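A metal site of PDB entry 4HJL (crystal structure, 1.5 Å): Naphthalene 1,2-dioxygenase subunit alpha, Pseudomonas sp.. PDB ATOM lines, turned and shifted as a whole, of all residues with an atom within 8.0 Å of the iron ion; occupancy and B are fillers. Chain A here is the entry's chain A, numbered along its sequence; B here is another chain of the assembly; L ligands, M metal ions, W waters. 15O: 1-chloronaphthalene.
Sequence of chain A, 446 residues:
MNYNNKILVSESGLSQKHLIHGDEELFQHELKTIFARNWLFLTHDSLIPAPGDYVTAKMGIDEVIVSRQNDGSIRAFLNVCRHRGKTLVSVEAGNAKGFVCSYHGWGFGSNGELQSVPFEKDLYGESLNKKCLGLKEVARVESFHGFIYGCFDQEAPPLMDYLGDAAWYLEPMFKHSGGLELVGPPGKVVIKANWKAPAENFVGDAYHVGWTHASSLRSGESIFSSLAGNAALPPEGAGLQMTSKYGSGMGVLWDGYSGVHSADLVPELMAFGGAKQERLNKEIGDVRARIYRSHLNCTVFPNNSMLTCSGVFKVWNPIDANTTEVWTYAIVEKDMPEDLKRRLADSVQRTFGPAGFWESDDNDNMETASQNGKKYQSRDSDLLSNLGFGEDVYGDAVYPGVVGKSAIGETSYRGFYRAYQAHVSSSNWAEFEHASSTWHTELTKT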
ATOM      1  N   ASN A 201       1.719  28.757 -30.387  1.00  0.00           N
ATOM      2  CA  ASN A 201       0.328  28.527 -30.748  1.00  0.00           C
ATOM      3  C   ASN A 201      -0.154  29.611 -31.711  1.00  0.00           C
ATOM      4  O   ASN A 201      -0.715  29.305 -32.768  1.00  0.00           O
ATOM      5  CB  ASN A 201      -0.518  28.449 -29.471  1.00  0.00           C
ATOM      6  CG  ASN A 201      -1.980  28.239 -29.737  1.00  0.00           C
ATOM      7  OD1 ASN A 201      -2.467  27.092 -29.779  1.00  0.00           O
ATOM      8  ND2 ASN A 201      -2.712  29.330 -29.906  1.00  0.00           N
ATOM      9  N   PHE A 202       0.100  30.876 -31.388  1.00  0.00           N
ATOM     10  CA  PHE A 202      -0.290  31.975 -32.282  1.00  0.00           C
ATOM     11  C   PHE A 202       0.526  32.038 -33.574  1.00  0.00           C
ATOM     12  O   PHE A 202       0.014  32.500 -34.593  1.00  0.00           O
ATOM     13  CB  PHE A 202      -0.236  33.325 -31.559  1.00  0.00           C
ATOM     14  CG  PHE A 202      -1.462  33.619 -30.722  1.00  0.00           C
ATOM     15  CD1 PHE A 202      -1.759  32.850 -29.605  1.00  0.00           C
ATOM     16  CD2 PHE A 202      -2.290  34.693 -31.030  1.00  0.00           C
ATOM     17  CE1 PHE A 202      -2.882  33.117 -28.826  1.00  0.00           C
ATOM     18  CE2 PHE A 202      -3.422  34.962 -30.249  1.00  0.00           C
ATOM     19  CZ  PHE A 202      -3.708  34.181 -29.155  1.00  0.00           C
ATOM     20  N   ASP A 205      -0.384  27.613 -35.256  1.00  0.00           N
ATOM     21  CA  ASP A 205      -1.247  26.503 -34.866  1.00  0.00           C
ATOM     22  C   ASP A 205      -2.699  26.696 -35.313  1.00  0.00           C
ATOM     23  O   ASP A 205      -3.536  27.140 -34.534  1.00  0.00           O
ATOM     24  CB  ASP A 205      -1.175  26.303 -33.359  1.00  0.00           C
ATOM     25  CG  ASP A 205      -1.810  25.009 -32.894  1.00  0.00           C
ATOM     26  OD1 ASP A 205      -2.542  24.344 -33.669  1.00  0.00           O
ATOM     27  OD2 ASP A 205      -1.602  24.669 -31.708  1.00  0.00           O
ATOM     28  N   HIS A 208      -5.108  23.242 -34.002  1.00  0.00           N
ATOM     29  CA  HIS A 208      -5.812  23.119 -32.722  1.00  0.00           C
ATOM     30  C   HIS A 208      -7.204  23.739 -32.713  1.00  0.00           C
ATOM     31  O   HIS A 208      -8.003  23.425 -31.850  1.00  0.00           O
ATOM     32  CB  HIS A 208      -4.988  23.722 -31.565  1.00  0.00           C
ATOM     33  CG  HIS A 208      -5.216  25.192 -31.343  1.00  0.00           C
ATOM     34  ND1 HIS A 208      -4.772  26.162 -32.215  1.00  0.00           N
ATOM     35  CD2 HIS A 208      -5.807  25.840 -30.318  1.00  0.00           C
ATOM     36  CE1 HIS A 208      -5.105  27.361 -31.746  1.00  0.00           C
ATOM     37  NE2 HIS A 208      -5.723  27.190 -30.590  1.00  0.00           N
ATOM     38  N   VAL A 209      -7.494  24.623 -33.660  1.00  0.00           N
ATOM     39  CA  VAL A 209      -8.684  25.468 -33.550  1.00  0.00           C
ATOM     40  C   VAL A 209     -10.011  24.705 -33.442  1.00  0.00           C
ATOM     41  O   VAL A 209     -10.786  24.922 -32.503  1.00  0.00           O
ATOM     42  CB  VAL A 209      -8.744  26.510 -34.677  1.00  0.00           C
ATOM     43  CG1 VAL A 209     -10.056  27.310 -34.634  1.00  0.00           C
ATOM     44  CG2 VAL A 209      -7.541  27.443 -34.604  1.00  0.00           C
ATOM     45  N   THR A 212      -9.634  22.272 -29.853  1.00  0.00           N
ATOM     46  CA  THR A 212      -9.498  23.095 -28.648  1.00  0.00           C
ATOM     47  C   THR A 212     -10.682  24.042 -28.469  1.00  0.00           C
ATOM     48  O   THR A 212     -11.239  24.139 -27.372  1.00  0.00           O
ATOM     49  CB  THR A 212      -8.194  23.921 -28.679  1.00  0.00           C
ATOM     50  OG1 THR A 212      -7.072  23.060 -28.499  1.00  0.00           O
ATOM     51  CG2 THR A 212      -8.175  24.963 -27.570  1.00  0.00           C
ATOM     52  N   HIS A 213     -11.062  24.709 -29.549  1.00  0.00           N
ATOM     53  CA  HIS A 213     -12.065  25.769 -29.470  1.00  0.00           C
ATOM     54  C   HIS A 213     -13.439  25.311 -29.924  1.00  0.00           C
ATOM     55  O   HIS A 213     -14.279  26.152 -30.250  1.00  0.00           O
ATOM     56  CB  HIS A 213     -11.623  27.005 -30.262  1.00  0.00           C
ATOM     57  CG  HIS A 213     -10.386  27.648 -29.710  1.00  0.00           C
ATOM     58  ND1 HIS A 213     -10.360  28.259 -28.476  1.00  0.00           N
ATOM     59  CD2 HIS A 213      -9.137  27.764 -30.222  1.00  0.00           C
ATOM     60  CE1 HIS A 213      -9.148  28.728 -28.250  1.00  0.00           C
ATOM     61  NE2 HIS A 213      -8.389  28.444 -29.282  1.00  0.00           N
ATOM     62  N   LEU A 307      -3.873  38.493 -33.681  1.00  0.00           N
ATOM     63  CA  LEU A 307      -4.820  37.995 -34.673  1.00  0.00           C
ATOM     64  C   LEU A 307      -5.333  39.227 -35.392  1.00  0.00           C
ATOM     65  O   LEU A 307      -6.113  39.983 -34.809  1.00  0.00           O
ATOM     66  CB  LEU A 307      -5.985  37.259 -34.018  1.00  0.00           C
ATOM     67  CG  LEU A 307      -5.644  36.104 -33.065  1.00  0.00           C
ATOM     68  CD1 LEU A 307      -6.918  35.471 -32.491  1.00  0.00           C
ATOM     69  CD2 LEU A 307      -4.786  35.039 -33.756  1.00  0.00           C
ATOM     70  N   PHE A 352     -10.859  36.940 -26.065  1.00  0.00           N
ATOM     71  CA  PHE A 352      -9.456  36.630 -25.768  1.00  0.00           C
ATOM     72  C   PHE A 352      -8.864  37.367 -24.566  1.00  0.00           C
ATOM     73  O   PHE A 352      -7.667  37.227 -24.302  1.00  0.00           O
ATOM     74  CB  PHE A 352      -8.586  36.829 -27.005  1.00  0.00           C
ATOM     75  CG  PHE A 352      -8.625  35.667 -27.953  1.00  0.00           C
ATOM     76  CD1 PHE A 352      -9.618  35.573 -28.909  1.00  0.00           C
ATOM     77  CD2 PHE A 352      -7.690  34.648 -27.851  1.00  0.00           C
ATOM     78  CE1 PHE A 352      -9.672  34.482 -29.764  1.00  0.00           C
ATOM     79  CE2 PHE A 352      -7.734  33.563 -28.714  1.00  0.00           C
ATOM     80  CZ  PHE A 352      -8.723  33.482 -29.666  1.00  0.00           C
ATOM     81  N   TRP A 358     -12.753  32.153 -25.544  1.00  0.00           N
ATOM     82  CA  TRP A 358     -11.867  31.412 -26.434  1.00  0.00           C
ATOM     83  C   TRP A 358     -10.525  31.157 -25.752  1.00  0.00           C
ATOM     84  O   TRP A 358     -10.032  30.028 -25.743  1.00  0.00           O
ATOM     85  CB  TRP A 358     -11.602  32.179 -27.739  1.00  0.00           C
ATOM     86  CG  TRP A 358     -12.767  32.276 -28.704  1.00  0.00           C
ATOM     87  CD1 TRP A 358     -13.954  32.938 -28.511  1.00  0.00           C
ATOM     88  CD2 TRP A 358     -12.805  31.775 -30.057  1.00  0.00           C
ATOM     89  NE1 TRP A 358     -14.738  32.838 -29.644  1.00  0.00           N
ATOM     90  CE2 TRP A 358     -14.052  32.135 -30.604  1.00  0.00           C
ATOM     91  CE3 TRP A 358     -11.911  31.045 -30.836  1.00  0.00           C
ATOM     92  CZ2 TRP A 358     -14.434  31.791 -31.906  1.00  0.00           C
ATOM     93  CZ3 TRP A 358     -12.280  30.702 -32.133  1.00  0.00           C
ATOM     94  CH2 TRP A 358     -13.534  31.079 -32.648  1.00  0.00           C
ATOM     95  N   GLU A 359      -9.914  32.201 -25.205  1.00  0.00           N
ATOM     96  CA  GLU A 359      -8.601  32.057 -24.597  1.00  0.00           C
ATOM     97  C   GLU A 359      -8.622  31.034 -23.466  1.00  0.00           C
ATOM     98  O   GLU A 359      -7.659  30.288 -23.265  1.00  0.00           O
ATOM     99  CB  GLU A 359      -8.070  33.423 -24.115  1.00  0.00           C
ATOM    100  CG  GLU A 359      -6.739  33.352 -23.382  1.00  0.00           C
ATOM    101  CD  GLU A 359      -5.613  34.021 -24.131  1.00  0.00           C
ATOM    102  OE1 GLU A 359      -5.627  34.020 -25.381  1.00  0.00           O
ATOM    103  OE2 GLU A 359      -4.691  34.566 -23.472  1.00  0.00           O
ATOM    104  N   SER A 360      -9.752  30.950 -22.760  1.00  0.00           N
ATOM    105  CA  SER A 360      -9.900  29.977 -21.688  1.00  0.00           C
ATOM    106  C   SER A 360      -9.772  28.532 -22.188  1.00  0.00           C
ATOM    107  O   SER A 360      -9.268  27.667 -21.457  1.00  0.00           O
ATOM    108  CB  SER A 360     -11.213  30.198 -20.921  1.00  0.00           C
ATOM    109  OG  SER A 360     -12.324  29.617 -21.595  1.00  0.00           O
ATOM    110  N   ASP A 361     -10.197  28.279 -23.429  1.00  0.00           N
ATOM    111  CA  ASP A 361     -10.101  26.942 -24.011  1.00  0.00           C
ATOM    112  C   ASP A 361      -8.648  26.475 -24.084  1.00  0.00           C
ATOM    113  O   ASP A 361      -8.385  25.283 -24.129  1.00  0.00           O
ATOM    114  CB  ASP A 361     -10.658  26.887 -25.438  1.00  0.00           C
ATOM    115  CG  ASP A 361     -12.118  27.290 -25.560  1.00  0.00           C
ATOM    116  OD1 ASP A 361     -12.907  27.129 -24.593  1.00  0.00           O
ATOM    117  OD2 ASP A 361     -12.487  27.742 -26.664  1.00  0.00           O
ATOM    118  N   ASP A 362      -7.724  27.442 -24.124  1.00  0.00           N
ATOM    119  CA  ASP A 362      -6.304  27.155 -24.336  1.00  0.00           C
ATOM    120  C   ASP A 362      -5.545  26.911 -23.043  1.00  0.00           C
ATOM    121  O   ASP A 362      -4.453  26.355 -23.087  1.00  0.00           O
ATOM    122  CB  ASP A 362      -5.597  28.313 -25.059  1.00  0.00           C
ATOM    123  CG  ASP A 362      -6.036  28.477 -26.499  1.00  0.00           C
ATOM    124  OD1 ASP A 362      -5.735  27.607 -27.346  1.00  0.00           O
ATOM    125  OD2 ASP A 362      -6.653  29.521 -26.807  1.00  0.00           O
ATOM    126  N   ASN A 363      -6.112  27.326 -21.898  1.00  0.00           N
ATOM    127  CA  ASN A 363      -5.377  27.309 -20.627  1.00  0.00           C
ATOM    128  C   ASN A 363      -4.729  25.972 -20.292  1.00  0.00           C
ATOM    129  O   ASN A 363      -3.523  25.899 -20.051  1.00  0.00           O
ATOM    130  CB  ASN A 363      -6.278  27.676 -19.435  1.00  0.00           C
ATOM    131  CG  ASN A 363      -6.559  29.156 -19.312  1.00  0.00           C
ATOM    132  OD1 ASN A 363      -7.318  29.556 -18.430  1.00  0.00           O
ATOM    133  ND2 ASN A 363      -5.977  29.981 -20.181  1.00  0.00           N
ATOM    134  N   ASN A 365      -4.232  23.328 -22.079  1.00  0.00           N
ATOM    135  CA  ASN A 365      -3.289  22.914 -23.113  1.00  0.00           C
ATOM    136  C   ASN A 365      -1.926  23.548 -22.890  1.00  0.00           C
ATOM    137  O   ASN A 365      -0.909  22.838 -22.875  1.00  0.00           O
ATOM    138  CB  ASN A 365      -3.810  23.252 -24.512  1.00  0.00           C
ATOM    139  CG  ASN A 365      -5.038  22.431 -24.901  1.00  0.00           C
ATOM    140  OD1 ASN A 365      -5.264  21.341 -24.385  1.00  0.00           O
ATOM    141  ND2 ASN A 365      -5.819  22.959 -25.838  1.00  0.00           N
ATOM    142  N   MET A 366      -1.887  24.868 -22.697  1.00  0.00           N
ATOM    143  CA  MET A 366      -0.607  25.567 -22.538  1.00  0.00           C
ATOM    144  C   MET A 366       0.062  25.259 -21.209  1.00  0.00           C
ATOM    145  O   MET A 366       1.280  25.086 -21.142  1.00  0.00           O
ATOM    146  CB  MET A 366      -0.721  27.092 -22.633  1.00  0.00           C
ATOM    147  CG  MET A 366      -1.947  27.651 -23.271  1.00  0.00           C
ATOM    148  SD  MET A 366      -1.475  28.758 -24.578  1.00  0.00           S
ATOM    149  CE  MET A 366      -0.504  27.554 -25.437  1.00  0.00           C
ATOM    150  N   TYR B 103      -5.893  19.055 -27.192  1.00  0.00           N
ATOM    151  CA  TYR B 103      -5.178  20.105 -27.904  1.00  0.00           C
ATOM    152  C   TYR B 103      -5.441  19.992 -29.417  1.00  0.00           C
ATOM    153  O   TYR B 103      -6.174  20.804 -29.982  1.00  0.00           O
ATOM    154  CB  TYR B 103      -3.685  20.084 -27.533  1.00  0.00           C
ATOM    155  CG  TYR B 103      -2.932  21.378 -27.778  1.00  0.00           C
ATOM    156  CD1 TYR B 103      -3.471  22.407 -28.546  1.00  0.00           C
ATOM    157  CD2 TYR B 103      -1.666  21.570 -27.245  1.00  0.00           C
ATOM    158  CE1 TYR B 103      -2.764  23.589 -28.777  1.00  0.00           C
ATOM    159  CE2 TYR B 103      -0.947  22.744 -27.467  1.00  0.00           C
ATOM    160  CZ  TYR B 103      -1.513  23.753 -28.236  1.00  0.00           C
ATOM    161  OH  TYR B 103      -0.820  24.924 -28.468  1.00  0.00           O
HETATM  162  C01 15O L   1      -4.134  30.916 -32.438  1.00  0.00           C
HETATM  163  C02 15O L   1      -5.319  31.521 -32.003  1.00  0.00           C
HETATM  164  C03 15O L   1      -6.386  31.674 -32.885  1.00  0.00           C
HETATM  165  C04 15O L   1      -6.268  31.226 -34.238  1.00  0.00           C
HETATM  166  C05 15O L   1      -5.107  30.633 -34.655  1.00  0.00           C
HETATM  167  C06 15O L   1      -4.012  30.469 -33.746  1.00  0.00           C
HETATM  168  C07 15O L   1      -4.969  30.167 -35.997  1.00  0.00           C
HETATM  169  C08 15O L   1      -6.029  30.323 -36.895  1.00  0.00           C
HETATM  170  C09 15O L   1      -7.209  30.930 -36.476  1.00  0.00           C
HETATM  171  C10 15O L   1      -7.353  31.378 -35.170  1.00  0.00           C
HETATM  172 CL1  15O L   1      -8.855  32.113 -34.709  1.00  0.00          CL
HETATM  173 FE    FE M   1      -6.336  28.585 -29.114  1.00  0.00          FE
HETATM  174  O   HOH W   1      -5.134  30.134 -29.291  1.00  0.00           O
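A ring nitrogen (ND1) of His 208 is in hydrogen-bond range of the backbone carbonyl oxygen (O) of Asp 205, at 2.8 Å.
ND1 of His 213 sits close to O of Trp 358, at 3.3 Å.
ND1 of His 213 sits at hydrogen-bond distance from OD2 of Asp 361.
ND1 of His 208 sits close to OD1 of Asn 201.
The side-chain amide oxygen (OD1) of Asn 201 sits at hydrogen-bond distance from the side-chain hydroxyl (OH) of Tyr 103 of chain B, at 3.0 Å.
OD2 of Asp 205 sits close to OD1 of Asn 201.
The backbone carbonyl oxygen (O) of His 208 sits close to the side-chain hydroxyl (OG1) of Thr 212 (3.5 Å).
Residues that only touch the iron ion: Asn 201 (3.8 Å).
Four residues have an atom within 4 Å of the iron ion: Asn 201, His 208, His 213 and Asp 362.
Along chain A the residues within 4 Å of the iron ion span positions 201 to 362.
The nearest printed residue that does not touch the iron ion is Thr 212 (4.3 Å).
Water W1 is bound to the iron ion, 2.0 Å away.
NE2 of His 213 binds the iron ion, at 2.1 Å.
OD1 of Asp 362 binds the iron ion (2.1 Å).
A ring nitrogen (NE2) of His 208 binds the iron ion (2.1 Å).
OD2 of Asp 362 binds the iron ion, at 2.5 Å.
The iron ion has five donor atoms within binding distance.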
